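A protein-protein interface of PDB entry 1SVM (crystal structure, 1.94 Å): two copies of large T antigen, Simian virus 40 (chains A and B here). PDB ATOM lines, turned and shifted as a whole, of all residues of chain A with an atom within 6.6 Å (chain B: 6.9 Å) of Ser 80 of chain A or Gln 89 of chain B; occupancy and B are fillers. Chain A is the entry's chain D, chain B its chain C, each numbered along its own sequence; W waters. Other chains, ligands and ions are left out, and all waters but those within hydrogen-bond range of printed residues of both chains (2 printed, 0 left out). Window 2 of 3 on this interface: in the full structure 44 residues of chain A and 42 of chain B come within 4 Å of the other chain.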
ATOM      1  N   GLN A  17      13.256 -21.250   4.104  1.00  0.00           N
ATOM      2  CA  GLN A  17      13.946 -21.878   5.227  1.00  0.00           C
ATOM      3  C   GLN A  17      15.376 -22.214   4.805  1.00  0.00           C
ATOM      4  O   GLN A  17      15.594 -22.769   3.729  1.00  0.00           O
ATOM      5  CB  GLN A  17      13.208 -23.157   5.634  1.00  0.00           C
ATOM      6  CG  GLN A  17      13.929 -24.013   6.664  1.00  0.00           C
ATOM      7  CD  GLN A  17      14.080 -23.318   8.002  1.00  0.00           C
ATOM      8  OE1 GLN A  17      13.092 -22.937   8.632  1.00  0.00           O
ATOM      9  NE2 GLN A  17      15.323 -23.154   8.447  1.00  0.00           N
ATOM     10  N   VAL A  18      16.351 -21.873   5.643  1.00  0.00           N
ATOM     11  CA  VAL A  18      17.743 -22.153   5.311  1.00  0.00           C
ATOM     12  C   VAL A  18      18.019 -23.645   5.258  1.00  0.00           C
ATOM     13  O   VAL A  18      17.485 -24.419   6.056  1.00  0.00           O
ATOM     14  CB  VAL A  18      18.728 -21.525   6.330  1.00  0.00           C
ATOM     15  CG1 VAL A  18      18.669 -20.017   6.247  1.00  0.00           C
ATOM     16  CG2 VAL A  18      18.397 -21.990   7.738  1.00  0.00           C
ATOM     17  N   TRP A  20      20.454 -26.296   6.080  1.00  0.00           N
ATOM     18  CA  TRP A  20      21.649 -26.558   6.876  1.00  0.00           C
ATOM     19  C   TRP A  20      22.587 -27.473   6.100  1.00  0.00           C
ATOM     20  O   TRP A  20      23.807 -27.313   6.142  1.00  0.00           O
ATOM     21  CB  TRP A  20      21.268 -27.225   8.195  1.00  0.00           C
ATOM     22  CG  TRP A  20      20.572 -26.329   9.164  1.00  0.00           C
ATOM     23  CD1 TRP A  20      19.543 -25.467   8.901  1.00  0.00           C
ATOM     24  CD2 TRP A  20      20.813 -26.247  10.572  1.00  0.00           C
ATOM     25  NE1 TRP A  20      19.127 -24.857  10.063  1.00  0.00           N
ATOM     26  CE2 TRP A  20      19.891 -25.319  11.102  1.00  0.00           C
ATOM     27  CE3 TRP A  20      21.720 -26.872  11.439  1.00  0.00           C
ATOM     28  CZ2 TRP A  20      19.848 -24.999  12.463  1.00  0.00           C
ATOM     29  CZ3 TRP A  20      21.679 -26.554  12.791  1.00  0.00           C
ATOM     30  CH2 TRP A  20      20.748 -25.625  13.289  1.00  0.00           C
ATOM     31  N   LEU A  39      31.480 -19.091   8.725  1.00  0.00           N
ATOM     32  CA  LEU A  39      30.471 -18.043   8.831  1.00  0.00           C
ATOM     33  C   LEU A  39      30.807 -16.869   7.917  1.00  0.00           C
ATOM     34  O   LEU A  39      29.949 -16.363   7.187  1.00  0.00           O
ATOM     35  CB  LEU A  39      30.366 -17.549  10.280  1.00  0.00           C
ATOM     36  CG  LEU A  39      29.402 -16.379  10.526  1.00  0.00           C
ATOM     37  CD1 LEU A  39      27.989 -16.781  10.117  1.00  0.00           C
ATOM     38  CD2 LEU A  39      29.439 -15.970  12.002  1.00  0.00           C
ATOM     39  N   ALA A  75      21.433 -16.070   0.790  1.00  0.00           N
ATOM     40  CA  ALA A  75      20.554 -14.921   0.957  1.00  0.00           C
ATOM     41  C   ALA A  75      19.639 -15.187   2.147  1.00  0.00           C
ATOM     42  O   ALA A  75      19.426 -14.312   2.980  1.00  0.00           O
ATOM     43  CB  ALA A  75      19.733 -14.696  -0.307  1.00  0.00           C
ATOM     44  N   ILE A  76      19.108 -16.405   2.226  1.00  0.00           N
ATOM     45  CA  ILE A  76      18.227 -16.790   3.322  1.00  0.00           C
ATOM     46  C   ILE A  76      19.033 -16.896   4.627  1.00  0.00           C
ATOM     47  O   ILE A  76      18.585 -16.443   5.683  1.00  0.00           O
ATOM     48  CB  ILE A  76      17.543 -18.148   3.034  1.00  0.00           C
ATOM     49  CG1 ILE A  76      16.840 -18.099   1.672  1.00  0.00           C
ATOM     50  CG2 ILE A  76      16.530 -18.470   4.133  1.00  0.00           C
ATOM     51  CD1 ILE A  76      16.228 -19.417   1.268  1.00  0.00           C
ATOM     52  N   PHE A  77      20.221 -17.495   4.540  1.00  0.00           N
ATOM     53  CA  PHE A  77      21.112 -17.654   5.693  1.00  0.00           C
ATOM     54  C   PHE A  77      21.355 -16.293   6.341  1.00  0.00           C
ATOM     55  O   PHE A  77      21.414 -16.175   7.563  1.00  0.00           O
ATOM     56  CB  PHE A  77      22.451 -18.261   5.235  1.00  0.00           C
ATOM     57  CG  PHE A  77      23.464 -18.433   6.340  1.00  0.00           C
ATOM     58  CD1 PHE A  77      23.477 -19.592   7.122  1.00  0.00           C
ATOM     59  CD2 PHE A  77      24.419 -17.446   6.589  1.00  0.00           C
ATOM     60  CE1 PHE A  77      24.430 -19.770   8.135  1.00  0.00           C
ATOM     61  CE2 PHE A  77      25.379 -17.611   7.602  1.00  0.00           C
ATOM     62  CZ  PHE A  77      25.384 -18.778   8.374  1.00  0.00           C
ATOM     63  N   ALA A  78      21.487 -15.262   5.509  1.00  0.00           N
ATOM     64  CA  ALA A  78      21.729 -13.906   5.988  1.00  0.00           C
ATOM     65  C   ALA A  78      20.615 -13.407   6.907  1.00  0.00           C
ATOM     66  O   ALA A  78      20.837 -12.521   7.736  1.00  0.00           O
ATOM     67  CB  ALA A  78      21.893 -12.960   4.803  1.00  0.00           C
ATOM     68  N   ASP A  79      19.418 -13.970   6.757  1.00  0.00           N
ATOM     69  CA  ASP A  79      18.280 -13.580   7.588  1.00  0.00           C
ATOM     70  C   ASP A  79      18.042 -14.529   8.753  1.00  0.00           C
ATOM     71  O   ASP A  79      17.123 -14.321   9.541  1.00  0.00           O
ATOM     72  CB  ASP A  79      16.997 -13.522   6.759  1.00  0.00           C
ATOM     73  CG  ASP A  79      17.036 -12.448   5.701  1.00  0.00           C
ATOM     74  OD1 ASP A  79      17.410 -11.305   6.033  1.00  0.00           O
ATOM     75  OD2 ASP A  79      16.687 -12.748   4.542  1.00  0.00           O
ATOM     76  N   SER A  80      18.859 -15.570   8.866  1.00  0.00           N
ATOM     77  CA  SER A  80      18.685 -16.541   9.944  1.00  0.00           C
ATOM     78  C   SER A  80      19.079 -16.024  11.320  1.00  0.00           C
ATOM     79  O   SER A  80      19.920 -15.130  11.447  1.00  0.00           O
ATOM     80  CB  SER A  80      19.483 -17.815   9.649  1.00  0.00           C
ATOM     81  OG  SER A  80      19.460 -18.687  10.772  1.00  0.00           O
ATOM     82  N   LYS A  81      18.465 -16.601  12.350  1.00  0.00           N
ATOM     83  CA  LYS A  81      18.753 -16.238  13.732  1.00  0.00           C
ATOM     84  C   LYS A  81      19.663 -17.281  14.391  1.00  0.00           C
ATOM     85  O   LYS A  81      20.001 -17.157  15.569  1.00  0.00           O
ATOM     86  CB  LYS A  81      17.454 -16.130  14.538  1.00  0.00           C
ATOM     87  CG  LYS A  81      16.504 -15.037  14.064  1.00  0.00           C
ATOM     88  CD  LYS A  81      15.236 -15.022  14.913  1.00  0.00           C
ATOM     89  CE  LYS A  81      14.326 -13.859  14.548  1.00  0.00           C
ATOM     90  NZ  LYS A  81      13.891 -13.904  13.125  1.00  0.00           N
ATOM     91  N   ASN A  82      20.058 -18.302  13.636  1.00  0.00           N
ATOM     92  CA  ASN A  82      20.915 -19.364  14.177  1.00  0.00           C
ATOM     93  C   ASN A  82      22.156 -19.587  13.327  1.00  0.00           C
ATOM     94  O   ASN A  82      22.618 -20.720  13.190  1.00  0.00           O
ATOM     95  CB  ASN A  82      20.152 -20.697  14.245  1.00  0.00           C
ATOM     96  CG  ASN A  82      18.850 -20.597  15.010  1.00  0.00           C
ATOM     97  OD1 ASN A  82      17.784 -20.383  14.428  1.00  0.00           O
ATOM     98  ND2 ASN A  82      18.929 -20.746  16.326  1.00  0.00           N
ATOM     99  N   GLN A  83      22.707 -18.515  12.772  1.00  0.00           N
ATOM    100  CA  GLN A  83      23.871 -18.626  11.899  1.00  0.00           C
ATOM    101  C   GLN A  83      25.024 -19.428  12.473  1.00  0.00           C
ATOM    102  O   GLN A  83      25.528 -20.339  11.821  1.00  0.00           O
ATOM    103  CB  GLN A  83      24.351 -17.233  11.489  1.00  0.00           C
ATOM    104  CG  GLN A  83      23.347 -16.513  10.605  1.00  0.00           C
ATOM    105  CD  GLN A  83      23.798 -15.130  10.200  1.00  0.00           C
ATOM    106  OE1 GLN A  83      23.217 -14.514   9.309  1.00  0.00           O
ATOM    107  NE2 GLN A  83      24.829 -14.624  10.864  1.00  0.00           N
ATOM    108  N   LYS A  84      25.434 -19.097  13.693  1.00  0.00           N
ATOM    109  CA  LYS A  84      26.544 -19.794  14.333  1.00  0.00           C
ATOM    110  C   LYS A  84      26.244 -21.281  14.544  1.00  0.00           C
ATOM    111  O   LYS A  84      27.092 -22.133  14.287  1.00  0.00           O
ATOM    112  CB  LYS A  84      26.865 -19.130  15.673  1.00  0.00           C
ATOM    113  CG  LYS A  84      28.197 -19.535  16.269  1.00  0.00           C
ATOM    114  CD  LYS A  84      28.480 -18.717  17.524  1.00  0.00           C
ATOM    115  CE  LYS A  84      29.901 -18.911  18.020  1.00  0.00           C
ATOM    116  NZ  LYS A  84      30.199 -17.986  19.154  1.00  0.00           N
ATOM    117  N   THR A  85      25.039 -21.584  15.013  1.00  0.00           N
ATOM    118  CA  THR A  85      24.640 -22.962  15.255  1.00  0.00           C
ATOM    119  C   THR A  85      24.700 -23.787  13.968  1.00  0.00           C
ATOM    120  O   THR A  85      25.176 -24.919  13.976  1.00  0.00           O
ATOM    121  CB  THR A  85      23.224 -23.023  15.842  1.00  0.00           C
ATOM    122  OG1 THR A  85      23.185 -22.229  17.030  1.00  0.00           O
ATOM    123  CG2 THR A  85      22.848 -24.453  16.203  1.00  0.00           C
ATOM    124  N   ILE A  86      24.217 -23.211  12.868  1.00  0.00           N
ATOM    125  CA  ILE A  86      24.240 -23.883  11.572  1.00  0.00           C
ATOM    126  C   ILE A  86      25.686 -24.176  11.167  1.00  0.00           C
ATOM    127  O   ILE A  86      26.007 -25.275  10.704  1.00  0.00           O
ATOM    128  CB  ILE A  86      23.589 -22.998  10.475  1.00  0.00           C
ATOM    129  CG1 ILE A  86      22.106 -22.802  10.782  1.00  0.00           C
ATOM    130  CG2 ILE A  86      23.769 -23.634   9.095  1.00  0.00           C
ATOM    131  CD1 ILE A  86      21.442 -21.730   9.921  1.00  0.00           C
ATOM    132  N   TRP B  20      17.501  -8.878  12.926  1.00  0.00           N
ATOM    133  CA  TRP B  20      18.835  -9.233  13.399  1.00  0.00           C
ATOM    134  C   TRP B  20      19.871  -8.742  12.402  1.00  0.00           C
ATOM    135  O   TRP B  20      20.967  -8.318  12.775  1.00  0.00           O
ATOM    136  CB  TRP B  20      18.964 -10.748  13.546  1.00  0.00           C
ATOM    137  CG  TRP B  20      18.211 -11.328  14.705  1.00  0.00           C
ATOM    138  CD1 TRP B  20      16.922 -11.057  15.068  1.00  0.00           C
ATOM    139  CD2 TRP B  20      18.681 -12.328  15.614  1.00  0.00           C
ATOM    140  NE1 TRP B  20      16.558 -11.830  16.145  1.00  0.00           N
ATOM    141  CE2 TRP B  20      17.620 -12.620  16.501  1.00  0.00           C
ATOM    142  CE3 TRP B  20      19.898 -13.009  15.767  1.00  0.00           C
ATOM    143  CZ2 TRP B  20      17.737 -13.566  17.529  1.00  0.00           C
ATOM    144  CZ3 TRP B  20      20.015 -13.952  16.792  1.00  0.00           C
ATOM    145  CH2 TRP B  20      18.939 -14.220  17.658  1.00  0.00           C
ATOM    146  N   LYS B  21      19.502  -8.804  11.127  1.00  0.00           N
ATOM    147  CA  LYS B  21      20.371  -8.393  10.035  1.00  0.00           C
ATOM    148  C   LYS B  21      20.754  -6.916  10.135  1.00  0.00           C
ATOM    149  O   LYS B  21      21.884  -6.542   9.826  1.00  0.00           O
ATOM    150  CB  LYS B  21      19.666  -8.686   8.707  1.00  0.00           C
ATOM    151  CG  LYS B  21      20.532  -8.619   7.468  1.00  0.00           C
ATOM    152  CD  LYS B  21      19.876  -9.420   6.347  1.00  0.00           C
ATOM    153  CE  LYS B  21      20.583  -9.227   5.020  1.00  0.00           C
ATOM    154  NZ  LYS B  21      20.356  -7.858   4.480  1.00  0.00           N
ATOM    155  N   THR B  24      23.339  -6.402  12.828  1.00  0.00           N
ATOM    156  CA  THR B  24      24.595  -6.915  12.293  1.00  0.00           C
ATOM    157  C   THR B  24      25.224  -5.901  11.341  1.00  0.00           C
ATOM    158  O   THR B  24      26.436  -5.679  11.366  1.00  0.00           O
ATOM    159  CB  THR B  24      24.366  -8.254  11.563  1.00  0.00           C
ATOM    160  OG1 THR B  24      23.929  -9.240  12.511  1.00  0.00           O
ATOM    161  CG2 THR B  24      25.647  -8.733  10.899  1.00  0.00           C
ATOM    162  N   VAL B  35      30.310  -7.053  22.366  1.00  0.00           N
ATOM    163  CA  VAL B  35      28.878  -7.231  22.584  1.00  0.00           C
ATOM    164  C   VAL B  35      28.207  -6.177  23.472  1.00  0.00           C
ATOM    165  O   VAL B  35      27.144  -5.666  23.120  1.00  0.00           O
ATOM    166  CB  VAL B  35      28.571  -8.636  23.140  1.00  0.00           C
ATOM    167  CG1 VAL B  35      27.071  -8.800  23.341  1.00  0.00           C
ATOM    168  CG2 VAL B  35      29.078  -9.693  22.168  1.00  0.00           C
ATOM    169  N   LEU B  38      28.118  -2.848  21.707  1.00  0.00           N
ATOM    170  CA  LEU B  38      27.091  -2.919  20.671  1.00  0.00           C
ATOM    171  C   LEU B  38      25.701  -2.729  21.266  1.00  0.00           C
ATOM    172  O   LEU B  38      24.888  -1.945  20.758  1.00  0.00           O
ATOM    173  CB  LEU B  38      27.158  -4.269  19.948  1.00  0.00           C
ATOM    174  CG  LEU B  38      26.126  -4.471  18.833  1.00  0.00           C
ATOM    175  CD1 LEU B  38      26.221  -3.325  17.819  1.00  0.00           C
ATOM    176  CD2 LEU B  38      26.362  -5.810  18.157  1.00  0.00           C
ATOM    177  N   LYS B  84      20.941  -9.577  24.043  1.00  0.00           N
ATOM    178  CA  LYS B  84      22.334 -10.011  24.022  1.00  0.00           C
ATOM    179  C   LYS B  84      22.600 -11.055  22.940  1.00  0.00           C
ATOM    180  O   LYS B  84      23.640 -11.019  22.281  1.00  0.00           O
ATOM    181  CB  LYS B  84      22.748 -10.558  25.394  1.00  0.00           C
ATOM    182  CG  LYS B  84      24.252 -10.773  25.523  1.00  0.00           C
ATOM    183  CD  LYS B  84      24.687 -11.012  26.960  1.00  0.00           C
ATOM    184  CE  LYS B  84      26.210 -10.970  27.074  1.00  0.00           C
ATOM    185  NZ  LYS B  84      26.698 -11.020  28.485  1.00  0.00           N
ATOM    186  N   THR B  85      21.663 -11.982  22.753  1.00  0.00           N
ATOM    187  CA  THR B  85      21.813 -13.018  21.736  1.00  0.00           C
ATOM    188  C   THR B  85      21.913 -12.379  20.351  1.00  0.00           C
ATOM    189  O   THR B  85      22.744 -12.777  19.529  1.00  0.00           O
ATOM    190  CB  THR B  85      20.615 -14.000  21.758  1.00  0.00           C
ATOM    191  OG1 THR B  85      20.558 -14.652  23.034  1.00  0.00           O
ATOM    192  CG2 THR B  85      20.764 -15.060  20.670  1.00  0.00           C
ATOM    193  N   ILE B  86      21.069 -11.387  20.093  1.00  0.00           N
ATOM    194  CA  ILE B  86      21.091 -10.700  18.806  1.00  0.00           C
ATOM    195  C   ILE B  86      22.438 -10.004  18.596  1.00  0.00           C
ATOM    196  O   ILE B  86      23.029 -10.077  17.516  1.00  0.00           O
ATOM    197  CB  ILE B  86      19.970  -9.643  18.717  1.00  0.00           C
ATOM    198  CG1 ILE B  86      18.601 -10.324  18.784  1.00  0.00           C
ATOM    199  CG2 ILE B  86      20.113  -8.841  17.425  1.00  0.00           C
ATOM    200  CD1 ILE B  86      17.437  -9.341  18.855  1.00  0.00           C
ATOM    201  N   CYS B  87      22.922  -9.335  19.634  1.00  0.00           N
ATOM    202  CA  CYS B  87      24.196  -8.639  19.553  1.00  0.00           C
ATOM    203  C   CYS B  87      25.344  -9.627  19.382  1.00  0.00           C
ATOM    204  O   CYS B  87      26.328  -9.330  18.705  1.00  0.00           O
ATOM    205  CB  CYS B  87      24.402  -7.777  20.801  1.00  0.00           C
ATOM    206  SG  CYS B  87      23.253  -6.370  20.882  1.00  0.00           S
ATOM    207  N   GLN B  88      25.210 -10.808  19.984  1.00  0.00           N
ATOM    208  CA  GLN B  88      26.238 -11.840  19.868  1.00  0.00           C
ATOM    209  C   GLN B  88      26.438 -12.255  18.415  1.00  0.00           C
ATOM    210  O   GLN B  88      27.567 -12.368  17.948  1.00  0.00           O
ATOM    211  CB  GLN B  88      25.858 -13.075  20.685  1.00  0.00           C
ATOM    212  CG  GLN B  88      26.535 -13.166  22.031  1.00  0.00           C
ATOM    213  CD  GLN B  88      28.052 -13.176  21.914  1.00  0.00           C
ATOM    214  OE1 GLN B  88      28.609 -13.698  20.947  1.00  0.00           O
ATOM    215  NE2 GLN B  88      28.726 -12.612  22.908  1.00  0.00           N
ATOM    216  N   GLN B  89      25.340 -12.500  17.706  1.00  0.00           N
ATOM    217  CA  GLN B  89      25.439 -12.895  16.310  1.00  0.00           C
ATOM    218  C   GLN B  89      26.028 -11.764  15.474  1.00  0.00           C
ATOM    219  O   GLN B  89      26.757 -12.009  14.512  1.00  0.00           O
ATOM    220  CB  GLN B  89      24.071 -13.289  15.752  1.00  0.00           C
ATOM    221  CG  GLN B  89      24.114 -13.626  14.266  1.00  0.00           C
ATOM    222  CD  GLN B  89      22.876 -14.359  13.788  1.00  0.00           C
ATOM    223  OE1 GLN B  89      22.650 -15.518  14.144  1.00  0.00           O
ATOM    224  NE2 GLN B  89      22.063 -13.686  12.981  1.00  0.00           N
ATOM    225  N   ALA B  90      25.703 -10.526  15.838  1.00  0.00           N
ATOM    226  CA  ALA B  90      26.224  -9.367  15.122  1.00  0.00           C
ATOM    227  C   ALA B  90      27.741  -9.313  15.315  1.00  0.00           C
ATOM    228  O   ALA B  90      28.494  -9.129  14.356  1.00  0.00           O
ATOM    229  CB  ALA B  90      25.579  -8.092  15.652  1.00  0.00           C
ATOM    230  N   VAL B  91      28.181  -9.479  16.561  1.00  0.00           N
ATOM    231  CA  VAL B  91      29.606  -9.454  16.872  1.00  0.00           C
ATOM    232  C   VAL B  91      30.352 -10.617  16.214  1.00  0.00           C
ATOM    233  O   VAL B  91      31.482 -10.450  15.756  1.00  0.00           O
ATOM    234  CB  VAL B  91      29.844  -9.482  18.406  1.00  0.00           C
ATOM    235  CG1 VAL B  91      31.259  -9.956  18.720  1.00  0.00           C
ATOM    236  CG2 VAL B  91      29.628  -8.079  18.985  1.00  0.00           C
ATOM    237  N   ASP B  92      29.729 -11.793  16.168  1.00  0.00           N
ATOM    238  CA  ASP B  92      30.369 -12.946  15.545  1.00  0.00           C
ATOM    239  C   ASP B  92      30.608 -12.721  14.059  1.00  0.00           C
ATOM    240  O   ASP B  92      31.585 -13.221  13.500  1.00  0.00           O
ATOM    241  CB  ASP B  92      29.534 -14.214  15.751  1.00  0.00           C
ATOM    242  CG  ASP B  92      29.584 -14.707  17.183  1.00  0.00           C
ATOM    243  OD1 ASP B  92      30.562 -14.373  17.889  1.00  0.00           O
ATOM    244  OD2 ASP B  92      28.657 -15.431  17.602  1.00  0.00           O
ATOM    245  N   THR B  93      29.707 -11.969  13.431  1.00  0.00           N
ATOM    246  CA  THR B  93      29.800 -11.637  12.011  1.00  0.00           C
ATOM    247  C   THR B  93      31.012 -10.735  11.776  1.00  0.00           C
ATOM    248  O   THR B  93      31.717 -10.863  10.772  1.00  0.00           O
ATOM    249  CB  THR B  93      28.526 -10.900  11.540  1.00  0.00           C
ATOM    250  OG1 THR B  93      27.391 -11.759  11.717  1.00  0.00           O
ATOM    251  CG2 THR B  93      28.636 -10.511  10.067  1.00  0.00           C
ATOM    252  N   VAL B  94      31.240  -9.814  12.709  1.00  0.00           N
ATOM    253  CA  VAL B  94      32.373  -8.901  12.621  1.00  0.00           C
ATOM    254  C   VAL B  94      33.653  -9.708  12.819  1.00  0.00           C
ATOM    255  O   VAL B  94      34.636  -9.521  12.098  1.00  0.00           O
ATOM    256  CB  VAL B  94      32.271  -7.791  13.695  1.00  0.00           C
ATOM    257  CG1 VAL B  94      33.549  -6.966  13.728  1.00  0.00           C
ATOM    258  CG2 VAL B  94      31.069  -6.908  13.401  1.00  0.00           C
HETATM  259  O   HOH W   1      25.400 -12.085  10.030  1.00  0.00           O
HETATM  260  O   HOH W   2      24.413 -17.000  15.379  1.00  0.00           O
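The backbone carbonyl oxygen of Ser 80 of chain A lies within hydrogen-bond range of the side-chain amide nitrogen of Gln 89 of chain B, 3.0 Å away.
The side-chain amide oxygen (OE1) of Gln 89 of chain B lies close to the backbone carbonyl oxygen (O) of Lys 81 of chain A (3.4 Å).
OE1 of Gln 89 of chain B is in hydrogen-bond range of N of Gln 83 of chain A (3.3 Å).
The side-chain carboxylate of Asp 92 of chain B lies within salt-bridge range of the side-chain amino group of Lys 84 of chain A (3.4 Å).
The backbone carbonyl oxygen (O) of Trp 20 of chain B sits at hydrogen-bond distance from the side-chain hydroxyl (OG1) of Thr 24 of chain B (3.1 Å).
The side-chain hydroxyl (OG1) of Thr 93 of chain B is in hydrogen-bond range of the backbone carbonyl oxygen (O) of Gln 89 of chain B, 2.9 Å away.
OE1 of Gln 83 of chain A sits close to O of Phe 77 of chain A (3.0 Å).
The backbone carbonyl oxygen (O) of Ala 78 of chain A lies close to the side-chain amide oxygen (OE1) of Gln 83 of chain A (3.5 Å).
The side-chain hydroxyl (OG) of Ser 80 of chain A sits at hydrogen-bond distance from the backbone NH (N) of Asn 82 of chain A (3.0 Å).
Leu 39 of chain A touches Asp 92 of chain B (CD2 to O, 3.8 Å).
Ala 78 of chain A touches Lys 21 of chain B.
CD of Lys 21 of chain B touches OD1 of Asp 79 of chain A, at 3.1 Å.
Lys 81 of chain A touches Trp 20 of chain B (CE to NE1, 3.4 Å).
Asn 82 of chain A touches Gln 89 of chain B (N to OE1, 3.8 Å).
OG1 of Thr 93 of chain B touches NE2 of Gln 83 of chain A (3.9 Å).
Ser 80 of chain A touches one residue of chain B.
Gln 89 of chain B touches just these residues of chain A: Ser 80, Lys 81, Asn 82 and Gln 83.
Of the printed residues of chain B, Asp 79 of chain A touches Lys 21.
Of the printed residues of chain B, Ala 78 of chain A touches Lys 21.
Of the printed residues of chain B, Gln 83 of chain A touches Gln 89 (3.3 Å) and Thr 93 (3.9 Å).
Ile 76 of chain A touches none of the printed residues of chain B.
The nearest residue of chain B that does not touch Ser 80 of chain A is Trp 20 of chain B (4.8 Å).
The nearest residue of chain A that does not touch Gln 89 of chain B is Lys 84 of chain A (4.6 Å).
The nearest printed residue of chain B that does not touch Gln 83 of chain A is Thr 24 of chain B (5.7 Å).
Of the 16 printed residues of chain A, 8 touch a printed residue of chain B.
Printed residues of chain B that touch a printed residue of chain A: Trp 20, Lys 21, Gln 89, Asp 92 and Thr 93.
Hydrophobic or aromatic side chains of chain B within 4 Å of the printed part of chain A: Trp 20.
Among the printed residues, 10 pairs touch across the chains.
Among the printed residues, Asp or Glu carboxylates within 4 Å of a Lys or Arg side-chain nitrogen of the other chain: Lys 84 of chain A with Asp 92 of chain B.
4 positions are printed for both chains.
Water W2 lies within hydrogen-bond range of the side-chain amide oxygen (OE1) of Gln 89 of chain B (2.6 Å), the backbone NH (N) of Lys 84 of chain A (2.9 Å) and the backbone NH (N) of Gln 83 of chain A (3.5 Å).
Water W1 lies within hydrogen-bond range of OG1 of Thr 93 of chain B and NE2 of Gln 83 of chain A.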
